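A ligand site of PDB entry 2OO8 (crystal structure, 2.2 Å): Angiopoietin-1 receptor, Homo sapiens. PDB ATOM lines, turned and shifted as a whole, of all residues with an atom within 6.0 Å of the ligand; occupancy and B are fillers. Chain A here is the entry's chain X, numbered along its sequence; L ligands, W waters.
A nitrogen (N2) of the ligand is in hydrogen-bond range of the side-chain carboxylate (OE2) of Glu 65, 2.9 Å away. The backbone NH (N) of Asp 175 lies within hydrogen-bond range of an oxygen (O1) of the ligand. O of Asp 175 lies within hydrogen-bond range of N2 of the ligand, at 3.4 Å. The side-chain carboxylate of Asp 175 is in salt-bridge range of a nitrogen (N1) of the ligand, 3.6 Å away. The backbone NH (N) of Ala 98 lies within hydrogen-bond range of a nitrogen (N5) of the ligand (3.0 Å).
The side-chain carboxylate of Glu 65 is in salt-bridge range of the side-chain amino group of Lys 48 (3.7 Å). OD1 of Asp 175 is in hydrogen-bond range of N of Gly 177. NE2 of His 155 lies within hydrogen-bond range of O of Ala 174 (2.7 Å). The backbone NH (N) of Phe 153 is in hydrogen-bond range of the backbone carbonyl oxygen (O) of Leu 148 (3.2 Å). The backbone carbonyl oxygen of Ile 173 sits at hydrogen-bond distance from the backbone NH of Ile 79. O of Ala 46 lies within hydrogen-bond range of N of Ile 95, 3.0 Å away. The backbone carbonyl oxygen of Leu 93 is in hydrogen-bond range of the backbone NH of Lys 48, at 2.8 Å.
NE2 of His 155 lies close to F1 of the ligand. A fluorine (F2) of the ligand lies close to the backbone carbonyl oxygen (O) of Ile 173. The backbone carbonyl oxygen (O) of Ala 174 sits close to a fluorine (F1) of the ligand (3.2 Å). Val 31 touches the ligand. Ala 46 touches the ligand (CB to N6, 3.5 Å). N of Lys 48 touches C19 of the ligand, 3.9 Å away. Leu 69 touches the ligand. Leu 72 touches the ligand. CG1 of Ile 79 touches F2 of the ligand (3.6 Å). Ile 95 touches the ligand (CD1 to C20, 3.6 Å). O of Glu 96 touches C29 of the ligand (3.7 Å). Tyr 97 touches the ligand. Phe 153 touches the ligand. Leu 164 touches the ligand (CD1 to C29, 3.7 Å). Phe 176 touches the ligand. Hydrophobic or aromatic side chains that line the ligand: Val 31, Ala 46, Leu 69, Leu 72, Ile 79, Ile 95, Tyr 97, Ala 98, Phe 153, His 155, Leu 164, Ile 173, Ala 174 and Phe 176. Of the 29 residues printed, 18 come within 4 Å of the ligand. The nearest printed residue that does not touch the ligand is Gly 177 (4.1 Å).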
ATOM      1  N   VAL A  31     -18.133   7.251  -1.003  1.00  0.00           N
ATOM      2  CA  VAL A  31     -19.497   7.734  -0.822  1.00  0.00           C
ATOM      3  C   VAL A  31     -19.672   8.581   0.451  1.00  0.00           C
ATOM      4  O   VAL A  31     -19.350   8.141   1.559  1.00  0.00           O
ATOM      5  CB  VAL A  31     -20.552   6.590  -0.876  1.00  0.00           C
ATOM      6  CG1 VAL A  31     -21.968   7.140  -0.797  1.00  0.00           C
ATOM      7  CG2 VAL A  31     -20.389   5.769  -2.140  1.00  0.00           C
ATOM      8  N   ALA A  46     -26.699  10.823  -1.436  1.00  0.00           N
ATOM      9  CA  ALA A  46     -25.455  10.080  -1.321  1.00  0.00           C
ATOM     10  C   ALA A  46     -24.735  10.236  -2.646  1.00  0.00           C
ATOM     11  O   ALA A  46     -25.335  10.054  -3.708  1.00  0.00           O
ATOM     12  CB  ALA A  46     -25.727   8.640  -1.021  1.00  0.00           C
ATOM     13  N   ILE A  47     -23.454  10.594  -2.598  1.00  0.00           N
ATOM     14  CA  ILE A  47     -22.680  10.865  -3.810  1.00  0.00           C
ATOM     15  C   ILE A  47     -21.423  10.022  -3.871  1.00  0.00           C
ATOM     16  O   ILE A  47     -20.614  10.025  -2.939  1.00  0.00           O
ATOM     17  CB  ILE A  47     -22.325  12.377  -3.986  1.00  0.00           C
ATOM     18  CG1 ILE A  47     -23.566  13.253  -3.796  1.00  0.00           C
ATOM     19  CG2 ILE A  47     -21.676  12.632  -5.352  1.00  0.00           C
ATOM     20  CD1 ILE A  47     -23.358  14.750  -4.076  1.00  0.00           C
ATOM     21  N   LYS A  48     -21.273   9.300  -4.978  1.00  0.00           N
ATOM     22  CA  LYS A  48     -20.080   8.500  -5.259  1.00  0.00           C
ATOM     23  C   LYS A  48     -19.007   9.409  -5.878  1.00  0.00           C
ATOM     24  O   LYS A  48     -19.220   9.970  -6.955  1.00  0.00           O
ATOM     25  CB  LYS A  48     -20.427   7.370  -6.221  1.00  0.00           C
ATOM     26  CG  LYS A  48     -19.336   6.315  -6.398  1.00  0.00           C
ATOM     27  CD  LYS A  48     -19.756   4.952  -5.865  1.00  0.00           C
ATOM     28  CE  LYS A  48     -20.712   4.255  -6.832  1.00  0.00           C
ATOM     29  NZ  LYS A  48     -20.804   2.789  -6.598  1.00  0.00           N
ATOM     30  N   GLY A  64     -20.169   2.902 -17.022  1.00  0.00           N
ATOM     31  CA  GLY A  64     -21.133   1.814 -17.202  1.00  0.00           C
ATOM     32  C   GLY A  64     -22.324   1.967 -16.283  1.00  0.00           C
ATOM     33  O   GLY A  64     -23.465   1.898 -16.719  1.00  0.00           O
ATOM     34  N   GLU A  65     -22.035   2.188 -15.001  1.00  0.00           N
ATOM     35  CA  GLU A  65     -23.054   2.399 -14.000  1.00  0.00           C
ATOM     36  C   GLU A  65     -23.964   3.574 -14.336  1.00  0.00           C
ATOM     37  O   GLU A  65     -25.185   3.433 -14.285  1.00  0.00           O
ATOM     38  CB  GLU A  65     -22.410   2.624 -12.641  1.00  0.00           C
ATOM     39  CG  GLU A  65     -23.402   2.874 -11.533  1.00  0.00           C
ATOM     40  CD  GLU A  65     -22.848   2.502 -10.186  1.00  0.00           C
ATOM     41  OE1 GLU A  65     -21.769   1.869 -10.130  1.00  0.00           O
ATOM     42  OE2 GLU A  65     -23.490   2.843  -9.185  1.00  0.00           O
ATOM     43  N   VAL A  68     -26.282   2.695 -17.129  1.00  0.00           N
ATOM     44  CA  VAL A  68     -27.383   1.863 -16.653  1.00  0.00           C
ATOM     45  C   VAL A  68     -28.446   2.703 -15.958  1.00  0.00           C
ATOM     46  O   VAL A  68     -29.607   2.665 -16.354  1.00  0.00           O
ATOM     47  CB  VAL A  68     -26.891   0.703 -15.721  1.00  0.00           C
ATOM     48  CG1 VAL A  68     -28.063   0.015 -15.049  1.00  0.00           C
ATOM     49  CG2 VAL A  68     -26.096  -0.311 -16.520  1.00  0.00           C
ATOM     50  N   LEU A  69     -28.031   3.491 -14.964  1.00  0.00           N
ATOM     51  CA  LEU A  69     -28.969   4.259 -14.140  1.00  0.00           C
ATOM     52  C   LEU A  69     -29.831   5.242 -14.940  1.00  0.00           C
ATOM     53  O   LEU A  69     -30.992   5.480 -14.577  1.00  0.00           O
ATOM     54  CB  LEU A  69     -28.249   4.967 -12.984  1.00  0.00           C
ATOM     55  CG  LEU A  69     -27.436   4.131 -11.978  1.00  0.00           C
ATOM     56  CD1 LEU A  69     -27.072   4.971 -10.764  1.00  0.00           C
ATOM     57  CD2 LEU A  69     -28.160   2.874 -11.528  1.00  0.00           C
ATOM     58  N   LEU A  72     -32.865   3.520 -16.480  1.00  0.00           N
ATOM     59  CA  LEU A  72     -33.806   2.923 -15.519  1.00  0.00           C
ATOM     60  C   LEU A  72     -35.074   3.726 -15.295  1.00  0.00           C
ATOM     61  O   LEU A  72     -36.083   3.177 -14.875  1.00  0.00           O
ATOM     62  CB  LEU A  72     -33.115   2.693 -14.183  1.00  0.00           C
ATOM     63  CG  LEU A  72     -32.008   1.641 -14.190  1.00  0.00           C
ATOM     64  CD1 LEU A  72     -31.621   1.334 -12.769  1.00  0.00           C
ATOM     65  CD2 LEU A  72     -32.459   0.389 -14.942  1.00  0.00           C
ATOM     66  N   ILE A  78     -37.255   1.792  -6.912  1.00  0.00           N
ATOM     67  CA  ILE A  78     -35.865   1.752  -7.382  1.00  0.00           C
ATOM     68  C   ILE A  78     -35.148   3.020  -6.910  1.00  0.00           C
ATOM     69  O   ILE A  78     -35.807   4.031  -6.628  1.00  0.00           O
ATOM     70  CB  ILE A  78     -35.749   1.636  -8.924  1.00  0.00           C
ATOM     71  CG1 ILE A  78     -36.331   2.885  -9.625  1.00  0.00           C
ATOM     72  CG2 ILE A  78     -36.403   0.365  -9.418  1.00  0.00           C
ATOM     73  CD1 ILE A  78     -35.625   3.268 -10.979  1.00  0.00           C
ATOM     74  N   ILE A  79     -33.823   2.971  -6.807  1.00  0.00           N
ATOM     75  CA  ILE A  79     -33.021   4.159  -6.455  1.00  0.00           C
ATOM     76  C   ILE A  79     -33.258   5.320  -7.436  1.00  0.00           C
ATOM     77  O   ILE A  79     -33.644   5.120  -8.585  1.00  0.00           O
ATOM     78  CB  ILE A  79     -31.485   3.872  -6.380  1.00  0.00           C
ATOM     79  CG1 ILE A  79     -30.945   3.358  -7.720  1.00  0.00           C
ATOM     80  CG2 ILE A  79     -31.166   2.980  -5.192  1.00  0.00           C
ATOM     81  CD1 ILE A  79     -29.555   3.806  -8.040  1.00  0.00           C
ATOM     82  N   LEU A  93     -21.381  10.990  -8.850  1.00  0.00           N
ATOM     83  CA  LEU A  93     -22.661  10.360  -9.188  1.00  0.00           C
ATOM     84  C   LEU A  93     -23.527  10.391  -7.945  1.00  0.00           C
ATOM     85  O   LEU A  93     -23.160   9.846  -6.914  1.00  0.00           O
ATOM     86  CB  LEU A  93     -22.410   8.912  -9.658  1.00  0.00           C
ATOM     87  CG  LEU A  93     -23.522   7.893  -9.955  1.00  0.00           C
ATOM     88  CD1 LEU A  93     -24.615   8.453 -10.859  1.00  0.00           C
ATOM     89  CD2 LEU A  93     -22.901   6.653 -10.597  1.00  0.00           C
ATOM     90  N   ALA A  94     -24.674  11.047  -8.040  1.00  0.00           N
ATOM     91  CA  ALA A  94     -25.507  11.264  -6.877  1.00  0.00           C
ATOM     92  C   ALA A  94     -26.872  10.591  -6.999  1.00  0.00           C
ATOM     93  O   ALA A  94     -27.539  10.690  -8.040  1.00  0.00           O
ATOM     94  CB  ALA A  94     -25.655  12.770  -6.604  1.00  0.00           C
ATOM     95  N   ILE A  95     -27.289   9.906  -5.934  1.00  0.00           N
ATOM     96  CA  ILE A  95     -28.667   9.389  -5.831  1.00  0.00           C
ATOM     97  C   ILE A  95     -29.361   9.923  -4.566  1.00  0.00           C
ATOM     98  O   ILE A  95     -28.699  10.311  -3.605  1.00  0.00           O
ATOM     99  CB  ILE A  95     -28.756   7.831  -5.883  1.00  0.00           C
ATOM    100  CG1 ILE A  95     -28.140   7.197  -4.638  1.00  0.00           C
ATOM    101  CG2 ILE A  95     -28.121   7.285  -7.176  1.00  0.00           C
ATOM    102  CD1 ILE A  95     -28.693   5.806  -4.319  1.00  0.00           C
ATOM    103  N   GLU A  96     -30.687   9.904  -4.556  1.00  0.00           N
ATOM    104  CA  GLU A  96     -31.425  10.321  -3.375  1.00  0.00           C
ATOM    105  C   GLU A  96     -31.022   9.486  -2.153  1.00  0.00           C
ATOM    106  O   GLU A  96     -30.814   8.276  -2.251  1.00  0.00           O
ATOM    107  CB  GLU A  96     -32.932  10.290  -3.608  1.00  0.00           C
ATOM    108  CG  GLU A  96     -33.736  10.848  -2.440  1.00  0.00           C
ATOM    109  CD  GLU A  96     -35.226  11.012  -2.713  1.00  0.00           C
ATOM    110  OE1 GLU A  96     -35.923  11.527  -1.807  1.00  0.00           O
ATOM    111  OE2 GLU A  96     -35.702  10.645  -3.812  1.00  0.00           O
ATOM    112  N   TYR A  97     -30.899  10.164  -1.014  1.00  0.00           N
ATOM    113  CA  TYR A  97     -30.444   9.556   0.226  1.00  0.00           C
ATOM    114  C   TYR A  97     -31.531   8.696   0.863  1.00  0.00           C
ATOM    115  O   TYR A  97     -32.733   9.022   0.794  1.00  0.00           O
ATOM    116  CB  TYR A  97     -29.958  10.628   1.226  1.00  0.00           C
ATOM    117  CG  TYR A  97     -29.185  10.050   2.403  1.00  0.00           C
ATOM    118  CD1 TYR A  97     -27.919   9.474   2.220  1.00  0.00           C
ATOM    119  CD2 TYR A  97     -29.721  10.049   3.695  1.00  0.00           C
ATOM    120  CE1 TYR A  97     -27.212   8.925   3.278  1.00  0.00           C
ATOM    121  CE2 TYR A  97     -29.013   9.501   4.783  1.00  0.00           C
ATOM    122  CZ  TYR A  97     -27.755   8.936   4.560  1.00  0.00           C
ATOM    123  OH  TYR A  97     -27.031   8.379   5.588  1.00  0.00           O
ATOM    124  N   ALA A  98     -31.099   7.594   1.484  1.00  0.00           N
ATOM    125  CA  ALA A  98     -31.993   6.701   2.215  1.00  0.00           C
ATOM    126  C   ALA A  98     -31.530   6.687   3.651  1.00  0.00           C
ATOM    127  O   ALA A  98     -30.481   6.100   3.967  1.00  0.00           O
ATOM    128  CB  ALA A  98     -31.983   5.302   1.622  1.00  0.00           C
ATOM    129  N   PRO A  99     -32.307   7.337   4.544  1.00  0.00           N
ATOM    130  CA  PRO A  99     -31.861   7.603   5.918  1.00  0.00           C
ATOM    131  C   PRO A  99     -31.861   6.351   6.792  1.00  0.00           C
ATOM    132  O   PRO A  99     -31.137   6.293   7.799  1.00  0.00           O
ATOM    133  CB  PRO A  99     -32.898   8.614   6.435  1.00  0.00           C
ATOM    134  CG  PRO A  99     -34.140   8.380   5.609  1.00  0.00           C
ATOM    135  CD  PRO A  99     -33.687   7.802   4.285  1.00  0.00           C
ATOM    136  N   GLY A 101     -30.889   3.291   5.781  1.00  0.00           N
ATOM    137  CA  GLY A 101     -29.857   2.350   5.352  1.00  0.00           C
ATOM    138  C   GLY A 101     -30.370   1.131   4.600  1.00  0.00           C
ATOM    139  O   GLY A 101     -31.533   1.092   4.164  1.00  0.00           O
ATOM    140  N   LEU A 148     -38.473  -3.036 -13.467  1.00  0.00           N
ATOM    141  CA  LEU A 148     -37.198  -3.237 -14.136  1.00  0.00           C
ATOM    142  C   LEU A 148     -37.206  -4.397 -15.139  1.00  0.00           C
ATOM    143  O   LEU A 148     -36.713  -4.264 -16.255  1.00  0.00           O
ATOM    144  CB  LEU A 148     -36.056  -3.435 -13.109  1.00  0.00           C
ATOM    145  CG  LEU A 148     -35.715  -2.292 -12.147  1.00  0.00           C
ATOM    146  CD1 LEU A 148     -34.615  -2.722 -11.158  1.00  0.00           C
ATOM    147  CD2 LEU A 148     -35.298  -1.014 -12.887  1.00  0.00           C
ATOM    148  N   PHE A 153     -34.267  -5.487 -17.897  1.00  0.00           N
ATOM    149  CA  PHE A 153     -33.178  -5.360 -16.940  1.00  0.00           C
ATOM    150  C   PHE A 153     -33.051  -6.639 -16.121  1.00  0.00           C
ATOM    151  O   PHE A 153     -34.048  -7.211 -15.660  1.00  0.00           O
ATOM    152  CB  PHE A 153     -33.420  -4.147 -16.031  1.00  0.00           C
ATOM    153  CG  PHE A 153     -32.389  -3.982 -14.954  1.00  0.00           C
ATOM    154  CD1 PHE A 153     -31.211  -3.273 -15.207  1.00  0.00           C
ATOM    155  CD2 PHE A 153     -32.590  -4.522 -13.692  1.00  0.00           C
ATOM    156  CE1 PHE A 153     -30.255  -3.106 -14.187  1.00  0.00           C
ATOM    157  CE2 PHE A 153     -31.647  -4.361 -12.682  1.00  0.00           C
ATOM    158  CZ  PHE A 153     -30.478  -3.648 -12.935  1.00  0.00           C
ATOM    159  N   HIS A 155     -30.968  -7.902 -12.740  1.00  0.00           N
ATOM    160  CA  HIS A 155     -30.256  -7.300 -11.629  1.00  0.00           C
ATOM    161  C   HIS A 155     -28.919  -7.996 -11.399  1.00  0.00           C
ATOM    162  O   HIS A 155     -27.872  -7.342 -11.405  1.00  0.00           O
ATOM    163  CB  HIS A 155     -31.078  -7.325 -10.336  1.00  0.00           C
ATOM    164  CG  HIS A 155     -30.460  -6.540  -9.230  1.00  0.00           C
ATOM    165  ND1 HIS A 155     -29.410  -7.007  -8.468  1.00  0.00           N
ATOM    166  CD2 HIS A 155     -30.716  -5.282  -8.772  1.00  0.00           C
ATOM    167  CE1 HIS A 155     -29.060  -6.095  -7.587  1.00  0.00           C
ATOM    168  NE2 HIS A 155     -29.840  -5.043  -7.742  1.00  0.00           N
ATOM    169  N   LEU A 164     -32.307  -0.565  -0.286  1.00  0.00           N
ATOM    170  CA  LEU A 164     -32.324   0.559   0.670  1.00  0.00           C
ATOM    171  C   LEU A 164     -33.715   0.767   1.283  1.00  0.00           C
ATOM    172  O   LEU A 164     -34.721   0.615   0.595  1.00  0.00           O
ATOM    173  CB  LEU A 164     -31.842   1.837  -0.022  1.00  0.00           C
ATOM    174  CG  LEU A 164     -30.337   1.863  -0.279  1.00  0.00           C
ATOM    175  CD1 LEU A 164     -29.974   2.922  -1.298  1.00  0.00           C
ATOM    176  CD2 LEU A 164     -29.576   2.064   1.037  1.00  0.00           C
ATOM    177  N   ILE A 173     -34.726  -0.867  -4.691  1.00  0.00           N
ATOM    178  CA  ILE A 173     -33.691  -1.701  -5.295  1.00  0.00           C
ATOM    179  C   ILE A 173     -32.457  -0.866  -5.596  1.00  0.00           C
ATOM    180  O   ILE A 173     -32.546   0.211  -6.158  1.00  0.00           O
ATOM    181  CB  ILE A 173     -34.202  -2.354  -6.592  1.00  0.00           C
ATOM    182  CG1 ILE A 173     -35.464  -3.180  -6.300  1.00  0.00           C
ATOM    183  CG2 ILE A 173     -33.096  -3.196  -7.248  1.00  0.00           C
ATOM    184  CD1 ILE A 173     -36.239  -3.455  -7.502  1.00  0.00           C
ATOM    185  N   ALA A 174     -31.303  -1.402  -5.216  1.00  0.00           N
ATOM    186  CA  ALA A 174     -30.021  -0.787  -5.519  1.00  0.00           C
ATOM    187  C   ALA A 174     -29.035  -1.887  -5.860  1.00  0.00           C
ATOM    188  O   ALA A 174     -29.399  -3.060  -5.958  1.00  0.00           O
ATOM    189  CB  ALA A 174     -29.532   0.018  -4.318  1.00  0.00           C
ATOM    190  N   ASP A 175     -27.781  -1.501  -6.062  1.00  0.00           N
ATOM    191  CA  ASP A 175     -26.705  -2.448  -6.313  1.00  0.00           C
ATOM    192  C   ASP A 175     -25.382  -1.789  -5.938  1.00  0.00           C
ATOM    193  O   ASP A 175     -24.915  -0.901  -6.664  1.00  0.00           O
ATOM    194  CB  ASP A 175     -26.690  -2.875  -7.788  1.00  0.00           C
ATOM    195  CG  ASP A 175     -25.722  -4.030  -8.076  1.00  0.00           C
ATOM    196  OD1 ASP A 175     -24.812  -4.327  -7.266  1.00  0.00           O
ATOM    197  OD2 ASP A 175     -25.863  -4.645  -9.147  1.00  0.00           O
ATOM    198  N   PHE A 176     -24.809  -2.212  -4.810  1.00  0.00           N
ATOM    199  CA  PHE A 176     -23.581  -1.593  -4.250  1.00  0.00           C
ATOM    200  C   PHE A 176     -22.294  -2.297  -4.699  1.00  0.00           C
ATOM    201  O   PHE A 176     -21.181  -1.832  -4.389  1.00  0.00           O
ATOM    202  CB  PHE A 176     -23.635  -1.541  -2.698  1.00  0.00           C
ATOM    203  CG  PHE A 176     -24.870  -0.871  -2.140  1.00  0.00           C
ATOM    204  CD1 PHE A 176     -25.792  -1.581  -1.375  1.00  0.00           C
ATOM    205  CD2 PHE A 176     -25.134   0.466  -2.416  1.00  0.00           C
ATOM    206  CE1 PHE A 176     -26.945  -0.976  -0.867  1.00  0.00           C
ATOM    207  CE2 PHE A 176     -26.289   1.094  -1.919  1.00  0.00           C
ATOM    208  CZ  PHE A 176     -27.196   0.368  -1.144  1.00  0.00           C
ATOM    209  N   GLY A 177     -22.444  -3.401  -5.419  1.00  0.00           N
ATOM    210  CA  GLY A 177     -21.309  -4.139  -5.941  1.00  0.00           C
ATOM    211  C   GLY A 177     -20.949  -5.364  -5.112  1.00  0.00           C
ATOM    212  O   GLY A 177     -21.430  -5.554  -3.985  1.00  0.00           O
ATOM    213  N   LEU A 178     -20.081  -6.190  -5.700  1.00  0.00           N
ATOM    214  CA  LEU A 178     -19.639  -7.437  -5.124  1.00  0.00           C
ATOM    215  C   LEU A 178     -18.348  -7.213  -4.340  1.00  0.00           C
ATOM    216  O   LEU A 178     -17.946  -8.059  -3.528  1.00  0.00           O
ATOM    217  CB  LEU A 178     -19.434  -8.478  -6.230  1.00  0.00           C
HETATM  218  C1  LIG L   1     -22.206  -3.327  -9.868  1.00  0.00           C
HETATM  219  N1  LIG L   1     -22.881  -3.914 -11.050  1.00  0.00           N
HETATM  220  C2  LIG L   1     -22.034  -3.883 -12.264  1.00  0.00           C
HETATM  221  C3  LIG L   1     -24.196  -3.270 -11.299  1.00  0.00           C
HETATM  222  C4  LIG L   1     -24.141  -1.759 -11.544  1.00  0.00           C
HETATM  223  C5  LIG L   1     -25.489  -1.278 -12.085  1.00  0.00           C
HETATM  224  C6  LIG L   1     -26.347  -0.661 -10.968  1.00  0.00           C
HETATM  225  C7  LIG L   1     -25.808   0.300 -10.096  1.00  0.00           C
HETATM  226  C8  LIG L   1     -27.676  -1.076 -10.821  1.00  0.00           C
HETATM  227  C9  LIG L   1     -28.486  -0.524  -9.803  1.00  0.00           C
HETATM  228  C10 LIG L   1     -29.948  -0.985  -9.630  1.00  0.00           C
HETATM  229  F1  LIG L   1     -29.975  -2.178  -9.028  1.00  0.00           F
HETATM  230  F2  LIG L   1     -30.615  -0.084  -8.871  1.00  0.00           F
HETATM  231  F3  LIG L   1     -30.564  -1.114 -10.803  1.00  0.00           F
HETATM  232  C11 LIG L   1     -27.935   0.442  -8.942  1.00  0.00           C
HETATM  233  C12 LIG L   1     -26.589   0.842  -9.068  1.00  0.00           C
HETATM  234  N2  LIG L   1     -26.072   1.806  -8.266  1.00  0.00           N
HETATM  235  C13 LIG L   1     -26.460   2.069  -7.011  1.00  0.00           C
HETATM  236  O1  LIG L   1     -27.297   1.427  -6.382  1.00  0.00           O
HETATM  237  C14 LIG L   1     -25.766   3.262  -6.305  1.00  0.00           C
HETATM  238  C15 LIG L   1     -25.919   3.403  -4.933  1.00  0.00           C
HETATM  239  C16 LIG L   1     -25.031   4.213  -7.022  1.00  0.00           C
HETATM  240  C17 LIG L   1     -24.424   5.287  -6.348  1.00  0.00           C
HETATM  241  C18 LIG L   1     -24.583   5.410  -4.955  1.00  0.00           C
HETATM  242  C19 LIG L   1     -23.920   6.604  -4.238  1.00  0.00           C
HETATM  243  C20 LIG L   1     -25.317   4.459  -4.237  1.00  0.00           C
HETATM  244  N3  LIG L   1     -25.526   4.566  -2.902  1.00  0.00           N
HETATM  245  C21 LIG L   1     -24.721   4.146  -1.933  1.00  0.00           C
HETATM  246  N4  LIG L   1     -23.608   3.480  -2.247  1.00  0.00           N
HETATM  247  C22 LIG L   1     -22.761   3.032  -1.328  1.00  0.00           C
HETATM  248  C23 LIG L   1     -23.034   3.226   0.026  1.00  0.00           C
HETATM  249  C24 LIG L   1     -24.198   3.893   0.412  1.00  0.00           C
HETATM  250  C25 LIG L   1     -25.056   4.374  -0.578  1.00  0.00           C
HETATM  251  C26 LIG L   1     -26.226   5.023  -0.161  1.00  0.00           C
HETATM  252  C27 LIG L   1     -26.520   5.161   1.186  1.00  0.00           C
HETATM  253  C28 LIG L   1     -27.695   5.799   1.563  1.00  0.00           C
HETATM  254  N5  LIG L   1     -28.520   6.250   0.633  1.00  0.00           N
HETATM  255  C29 LIG L   1     -28.244   6.090  -0.652  1.00  0.00           C
HETATM  256  N6  LIG L   1     -27.132   5.484  -1.048  1.00  0.00           N
HETATM  257  O   HOH W   1     -24.369  -6.469 -12.712  1.00  0.00           O
